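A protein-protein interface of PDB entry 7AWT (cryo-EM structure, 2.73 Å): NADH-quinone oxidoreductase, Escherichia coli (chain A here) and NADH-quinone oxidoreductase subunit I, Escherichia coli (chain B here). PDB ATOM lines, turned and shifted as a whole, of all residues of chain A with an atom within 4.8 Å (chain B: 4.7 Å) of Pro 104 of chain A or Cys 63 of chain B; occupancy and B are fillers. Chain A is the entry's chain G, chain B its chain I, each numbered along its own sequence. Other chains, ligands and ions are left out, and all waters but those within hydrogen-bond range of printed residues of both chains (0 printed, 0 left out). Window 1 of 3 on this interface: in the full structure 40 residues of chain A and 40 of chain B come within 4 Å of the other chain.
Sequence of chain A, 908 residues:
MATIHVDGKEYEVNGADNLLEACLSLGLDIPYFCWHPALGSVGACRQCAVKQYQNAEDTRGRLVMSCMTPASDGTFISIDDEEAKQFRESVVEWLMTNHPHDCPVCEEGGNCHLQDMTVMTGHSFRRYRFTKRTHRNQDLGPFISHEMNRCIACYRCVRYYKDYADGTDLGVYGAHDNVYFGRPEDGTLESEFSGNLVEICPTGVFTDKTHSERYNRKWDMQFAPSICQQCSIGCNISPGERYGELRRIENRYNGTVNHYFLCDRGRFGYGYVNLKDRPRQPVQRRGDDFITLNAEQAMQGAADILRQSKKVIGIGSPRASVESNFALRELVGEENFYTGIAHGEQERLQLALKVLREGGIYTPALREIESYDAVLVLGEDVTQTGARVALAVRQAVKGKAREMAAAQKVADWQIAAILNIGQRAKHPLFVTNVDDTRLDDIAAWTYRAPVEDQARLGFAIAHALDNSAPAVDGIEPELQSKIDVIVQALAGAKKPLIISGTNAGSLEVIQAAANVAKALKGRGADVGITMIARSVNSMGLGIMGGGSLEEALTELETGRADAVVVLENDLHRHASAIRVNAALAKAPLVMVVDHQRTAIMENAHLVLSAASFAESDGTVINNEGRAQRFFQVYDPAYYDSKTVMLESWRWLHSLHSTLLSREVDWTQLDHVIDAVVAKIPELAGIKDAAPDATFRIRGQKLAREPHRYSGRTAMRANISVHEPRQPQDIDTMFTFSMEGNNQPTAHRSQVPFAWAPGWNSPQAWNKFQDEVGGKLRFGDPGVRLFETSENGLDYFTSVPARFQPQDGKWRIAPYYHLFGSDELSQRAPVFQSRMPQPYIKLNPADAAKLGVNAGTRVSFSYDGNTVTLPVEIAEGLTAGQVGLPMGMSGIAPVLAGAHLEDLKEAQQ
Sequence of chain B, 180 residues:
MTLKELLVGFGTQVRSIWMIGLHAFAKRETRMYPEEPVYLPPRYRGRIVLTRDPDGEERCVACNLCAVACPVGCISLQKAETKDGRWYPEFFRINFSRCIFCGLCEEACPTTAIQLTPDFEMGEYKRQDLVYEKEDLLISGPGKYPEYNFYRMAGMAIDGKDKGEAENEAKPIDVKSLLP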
ATOM      1  N   HIS A 101      -4.883   5.471   8.228  1.00  0.00           N
ATOM      2  CA  HIS A 101      -4.634   4.806   9.471  1.00  0.00           C
ATOM      3  C   HIS A 101      -5.561   3.673   9.787  1.00  0.00           C
ATOM      4  O   HIS A 101      -6.116   3.612  10.824  1.00  0.00           O
ATOM      5  CB  HIS A 101      -4.756   5.836  10.561  1.00  0.00           C
ATOM      6  CG  HIS A 101      -4.317   5.357  11.892  1.00  0.00           C
ATOM      7  ND1 HIS A 101      -3.018   5.421  12.286  1.00  0.00           N
ATOM      8  CD2 HIS A 101      -4.996   4.833  12.927  1.00  0.00           C
ATOM      9  CE1 HIS A 101      -2.909   4.945  13.506  1.00  0.00           C
ATOM     10  NE2 HIS A 101      -4.100   4.580  13.916  1.00  0.00           N
ATOM     11  N   ASP A 102      -5.721   2.724   8.920  1.00  0.00           N
ATOM     12  CA  ASP A 102      -6.639   1.643   9.182  1.00  0.00           C
ATOM     13  C   ASP A 102      -6.200   0.219   8.968  1.00  0.00           C
ATOM     14  O   ASP A 102      -6.801  -0.507   8.258  1.00  0.00           O
ATOM     15  CB  ASP A 102      -7.918   1.876   8.420  1.00  0.00           C
ATOM     16  CG  ASP A 102      -7.742   1.768   6.987  1.00  0.00           C
ATOM     17  OD1 ASP A 102      -6.667   1.370   6.577  1.00  0.00           O
ATOM     18  OD2 ASP A 102      -8.661   2.103   6.251  1.00  0.00           O
ATOM     19  N   CYS A 103      -5.156  -0.195   9.629  1.00  0.00           N
ATOM     20  CA  CYS A 103      -4.722  -1.560   9.545  1.00  0.00           C
ATOM     21  C   CYS A 103      -5.682  -2.439  10.233  1.00  0.00           C
ATOM     22  O   CYS A 103      -5.937  -3.496   9.758  1.00  0.00           O
ATOM     23  CB  CYS A 103      -3.342  -1.769  10.119  1.00  0.00           C
ATOM     24  SG  CYS A 103      -2.060  -1.540   8.935  1.00  0.00           S
ATOM     25  N   PRO A 104      -6.204  -2.005  11.377  1.00  0.00           N
ATOM     26  CA  PRO A 104      -7.117  -2.790  12.177  1.00  0.00           C
ATOM     27  C   PRO A 104      -8.368  -3.131  11.449  1.00  0.00           C
ATOM     28  O   PRO A 104      -8.844  -4.191  11.597  1.00  0.00           O
ATOM     29  CB  PRO A 104      -7.429  -1.871  13.291  1.00  0.00           C
ATOM     30  CG  PRO A 104      -6.235  -1.096  13.475  1.00  0.00           C
ATOM     31  CD  PRO A 104      -5.693  -0.872  12.136  1.00  0.00           C
ATOM     32  N   VAL A 105      -8.908  -2.204  10.685  1.00  0.00           N
ATOM     33  CA  VAL A 105     -10.049  -2.422   9.857  1.00  0.00           C
ATOM     34  C   VAL A 105      -9.760  -2.816   8.405  1.00  0.00           C
ATOM     35  O   VAL A 105     -10.654  -2.971   7.676  1.00  0.00           O
ATOM     36  CB  VAL A 105     -10.989  -1.259   9.971  1.00  0.00           C
ATOM     37  CG1 VAL A 105     -11.250  -0.987  11.411  1.00  0.00           C
ATOM     38  CG2 VAL A 105     -10.310  -0.054   9.486  1.00  0.00           C
ATOM     39  N   CYS A 106      -8.520  -2.944   7.974  1.00  0.00           N
ATOM     40  CA  CYS A 106      -8.183  -3.419   6.629  1.00  0.00           C
ATOM     41  C   CYS A 106      -8.482  -4.906   6.514  1.00  0.00           C
ATOM     42  O   CYS A 106      -8.205  -5.664   7.432  1.00  0.00           O
ATOM     43  CB  CYS A 106      -6.719  -3.138   6.291  1.00  0.00           C
ATOM     44  SG  CYS A 106      -6.318  -3.176   4.525  1.00  0.00           S
ATOM     45  N   ARG A 217      -8.425 -13.228  10.352  1.00  0.00           N
ATOM     46  CA  ARG A 217      -7.084 -12.841   9.971  1.00  0.00           C
ATOM     47  C   ARG A 217      -6.335 -13.988   9.431  1.00  0.00           C
ATOM     48  O   ARG A 217      -6.687 -15.062   9.669  1.00  0.00           O
ATOM     49  CB  ARG A 217      -6.369 -12.269  11.132  1.00  0.00           C
ATOM     50  CG  ARG A 217      -6.944 -10.991  11.616  1.00  0.00           C
ATOM     51  CD  ARG A 217      -6.466  -9.889  10.745  1.00  0.00           C
ATOM     52  NE  ARG A 217      -6.893  -8.613  11.234  1.00  0.00           N
ATOM     53  CZ  ARG A 217      -7.092  -7.593  10.451  1.00  0.00           C
ATOM     54  NH1 ARG A 217      -7.480  -6.465  10.930  1.00  0.00           N
ATOM     55  NH2 ARG A 217      -6.936  -7.722   9.189  1.00  0.00           N
ATOM     56  N   TRP A 219      -3.569 -15.505  10.206  1.00  0.00           N
ATOM     57  CA  TRP A 219      -3.035 -16.456  11.157  1.00  0.00           C
ATOM     58  C   TRP A 219      -4.069 -17.401  11.664  1.00  0.00           C
ATOM     59  O   TRP A 219      -3.773 -18.549  11.854  1.00  0.00           O
ATOM     60  CB  TRP A 219      -2.309 -15.788  12.305  1.00  0.00           C
ATOM     61  CG  TRP A 219      -2.995 -14.674  12.912  1.00  0.00           C
ATOM     62  CD1 TRP A 219      -3.854 -14.723  13.936  1.00  0.00           C
ATOM     63  CD2 TRP A 219      -2.853 -13.305  12.573  1.00  0.00           C
ATOM     64  NE1 TRP A 219      -4.278 -13.469  14.263  1.00  0.00           N
ATOM     65  CE2 TRP A 219      -3.676 -12.579  13.426  1.00  0.00           C
ATOM     66  CE3 TRP A 219      -2.118 -12.623  11.622  1.00  0.00           C
ATOM     67  CZ2 TRP A 219      -3.783 -11.214  13.356  1.00  0.00           C
ATOM     68  CZ3 TRP A 219      -2.223 -11.281  11.558  1.00  0.00           C
ATOM     69  CH2 TRP A 219      -3.043 -10.584  12.418  1.00  0.00           C
ATOM     70  N   VAL B  61     -13.028  -3.238  17.235  1.00  0.00           N
ATOM     71  CA  VAL B  61     -13.295  -3.306  15.814  1.00  0.00           C
ATOM     72  C   VAL B  61     -13.081  -4.714  15.268  1.00  0.00           C
ATOM     73  O   VAL B  61     -13.133  -4.941  14.089  1.00  0.00           O
ATOM     74  CB  VAL B  61     -12.525  -2.262  15.022  1.00  0.00           C
ATOM     75  CG1 VAL B  61     -12.743  -0.914  15.649  1.00  0.00           C
ATOM     76  CG2 VAL B  61     -11.067  -2.582  15.016  1.00  0.00           C
ATOM     77  N   ALA B  62     -12.827  -5.659  16.144  1.00  0.00           N
ATOM     78  CA  ALA B  62     -12.656  -7.056  15.757  1.00  0.00           C
ATOM     79  C   ALA B  62     -11.567  -7.270  14.713  1.00  0.00           C
ATOM     80  O   ALA B  62     -11.848  -7.716  13.608  1.00  0.00           O
ATOM     81  CB  ALA B  62     -13.973  -7.635  15.273  1.00  0.00           C
ATOM     82  N   CYS B  63     -10.332  -6.932  15.067  1.00  0.00           N
ATOM     83  CA  CYS B  63      -9.188  -7.101  14.227  1.00  0.00           C
ATOM     84  C   CYS B  63      -8.357  -8.284  14.582  1.00  0.00           C
ATOM     85  O   CYS B  63      -7.471  -8.606  13.856  1.00  0.00           O
ATOM     86  CB  CYS B  63      -8.287  -5.911  14.335  1.00  0.00           C
ATOM     87  SG  CYS B  63      -8.079  -5.168  15.944  1.00  0.00           S
ATOM     88  N   ASN B  64      -8.641  -8.878  15.736  1.00  0.00           N
ATOM     89  CA  ASN B  64      -7.970 -10.048  16.276  1.00  0.00           C
ATOM     90  C   ASN B  64      -6.569  -9.820  16.742  1.00  0.00           C
ATOM     91  O   ASN B  64      -5.823 -10.753  16.851  1.00  0.00           O
ATOM     92  CB  ASN B  64      -7.929 -11.169  15.267  1.00  0.00           C
ATOM     93  CG  ASN B  64      -9.269 -11.785  15.033  1.00  0.00           C
ATOM     94  OD1 ASN B  64     -10.137 -11.700  15.867  1.00  0.00           O
ATOM     95  ND2 ASN B  64      -9.445 -12.405  13.889  1.00  0.00           N
ATOM     96  N   LEU B  65      -6.203  -8.600  17.054  1.00  0.00           N
ATOM     97  CA  LEU B  65      -4.838  -8.298  17.457  1.00  0.00           C
ATOM     98  C   LEU B  65      -4.598  -8.705  18.896  1.00  0.00           C
ATOM     99  O   LEU B  65      -3.467  -8.948  19.296  1.00  0.00           O
ATOM    100  CB  LEU B  65      -4.510  -6.820  17.274  1.00  0.00           C
ATOM    101  CG  LEU B  65      -4.007  -6.416  15.892  1.00  0.00           C
ATOM    102  CD1 LEU B  65      -3.226  -5.121  16.003  1.00  0.00           C
ATOM    103  CD2 LEU B  65      -3.126  -7.511  15.321  1.00  0.00           C
ATOM    104  N   TRP B  87     -16.993  -1.827  11.568  1.00  0.00           N
ATOM    105  CA  TRP B  87     -16.587  -3.119  12.096  1.00  0.00           C
ATOM    106  C   TRP B  87     -16.896  -3.191  13.584  1.00  0.00           C
ATOM    107  O   TRP B  87     -16.747  -2.206  14.309  1.00  0.00           O
ATOM    108  CB  TRP B  87     -15.093  -3.349  11.881  1.00  0.00           C
ATOM    109  CG  TRP B  87     -14.700  -3.696  10.493  1.00  0.00           C
ATOM    110  CD1 TRP B  87     -15.255  -3.229   9.343  1.00  0.00           C
ATOM    111  CD2 TRP B  87     -13.651  -4.584  10.100  1.00  0.00           C
ATOM    112  NE1 TRP B  87     -14.619  -3.774   8.257  1.00  0.00           N
ATOM    113  CE2 TRP B  87     -13.629  -4.610   8.698  1.00  0.00           C
ATOM    114  CE3 TRP B  87     -12.727  -5.361  10.802  1.00  0.00           C
ATOM    115  CZ2 TRP B  87     -12.725  -5.385   7.982  1.00  0.00           C
ATOM    116  CZ3 TRP B  87     -11.830  -6.126  10.090  1.00  0.00           C
ATOM    117  CH2 TRP B  87     -11.835  -6.133   8.696  1.00  0.00           C
ATOM    118  N   PRO B 110      -5.124  -1.845  19.433  1.00  0.00           N
ATOM    119  CA  PRO B 110      -4.845  -0.577  18.762  1.00  0.00           C
ATOM    120  C   PRO B 110      -6.021   0.383  18.846  1.00  0.00           C
ATOM    121  O   PRO B 110      -5.891   1.533  18.438  1.00  0.00           O
ATOM    122  CB  PRO B 110      -4.651  -1.004  17.314  1.00  0.00           C
ATOM    123  CG  PRO B 110      -5.568  -2.165  17.161  1.00  0.00           C
ATOM    124  CD  PRO B 110      -5.614  -2.864  18.491  1.00  0.00           C
ATOM    125  N   THR B 111      -7.153  -0.081  19.366  1.00  0.00           N
ATOM    126  CA  THR B 111      -8.333   0.766  19.476  1.00  0.00           C
ATOM    127  C   THR B 111      -8.762   1.029  20.911  1.00  0.00           C
ATOM    128  O   THR B 111      -9.831   1.585  21.135  1.00  0.00           O
ATOM    129  CB  THR B 111      -9.529   0.188  18.708  1.00  0.00           C
ATOM    130  OG1 THR B 111     -10.168  -0.810  19.506  1.00  0.00           O
ATOM    131  CG2 THR B 111      -9.079  -0.418  17.398  1.00  0.00           C
ATOM    132  N   PHE B 150     -10.796   5.711  17.721  1.00  0.00           N
ATOM    133  CA  PHE B 150     -10.040   5.137  16.613  1.00  0.00           C
ATOM    134  C   PHE B 150     -10.634   5.542  15.276  1.00  0.00           C
ATOM    135  O   PHE B 150      -9.912   5.941  14.357  1.00  0.00           O
ATOM    136  CB  PHE B 150      -9.994   3.617  16.730  1.00  0.00           C
ATOM    137  CG  PHE B 150      -9.483   2.935  15.496  1.00  0.00           C
ATOM    138  CD1 PHE B 150      -8.131   2.904  15.219  1.00  0.00           C
ATOM    139  CD2 PHE B 150     -10.351   2.325  14.615  1.00  0.00           C
ATOM    140  CE1 PHE B 150      -7.660   2.281  14.088  1.00  0.00           C
ATOM    141  CE2 PHE B 150      -9.882   1.702  13.486  1.00  0.00           C
ATOM    142  CZ  PHE B 150      -8.537   1.681  13.222  1.00  0.00           C
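NE of Arg 217 of chain A is in hydrogen-bond range of O of Cys 63 of chain B (2.7 Å).
O of Pro 104 of chain A is in hydrogen-bond range of NH1 of Arg 217 of chain A, 2.7 Å away.
The backbone carbonyl oxygen of Cys 106 of chain A sits at hydrogen-bond distance from the guanidinium group of Arg 217 of chain A (3.0 Å).
His 101 of chain A touches Phe 150 of chain B.
Pro 104 of chain A touches Cys 63 of chain B (O to CB, 3.3 Å).
Pro 104 of chain A touches Trp 87 of chain B.
Pro 104 of chain A touches Pro 110 of chain B (CG to CG, 3.9 Å).
Phe 150 of chain B touches Pro 104 of chain A (CZ to CG, 3.6 Å).
Val 105 of chain A touches Val 61 of chain B (CG1 to CG2, 3.9 Å).
Val 105 of chain A touches Trp 87 of chain B (O to CZ2, 3.2 Å).
Phe 150 of chain B touches Val 105 of chain A.
Cys 106 of chain A touches Trp 87 of chain B (O to CH2, 3.9 Å).
CG of Arg 217 of chain A touches ND2 of Asn 64 of chain B (3.7 Å).
Cys 63 of chain B touches just these residues of chain A: Pro 104 and Arg 217.
Of the printed residues of chain A, Asn 64 of chain B touches Arg 217.
Printed residues of chain A within 4 Å of Val 61 of chain B: Val 105 (3.9 Å).
Of the printed residues of chain B, His 101 of chain A touches Phe 150 (3.8 Å).
The nearest residue of chain B that does not touch Pro 104 of chain A is Val 61 of chain B (4.1 Å).
The nearest printed residue of chain B that does not touch Val 105 of chain A is Cys 63 of chain B (5.2 Å).
Printed residues of chain B that touch a printed residue of chain A: Val 61, Cys 63, Asn 64, Trp 87, Pro 110 and Phe 150.
Hydrophobic or aromatic side chains of chain B that line the printed part of chain A: Val 61, Trp 87, Pro 110 and Phe 150.
Along chain A the printed residues that touch a printed residue of chain B span positions 101 to 217.
Among the printed residues, no Asp or Glu carboxylate lies within 4 Å of a Lys or Arg side-chain nitrogen of the other chain.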
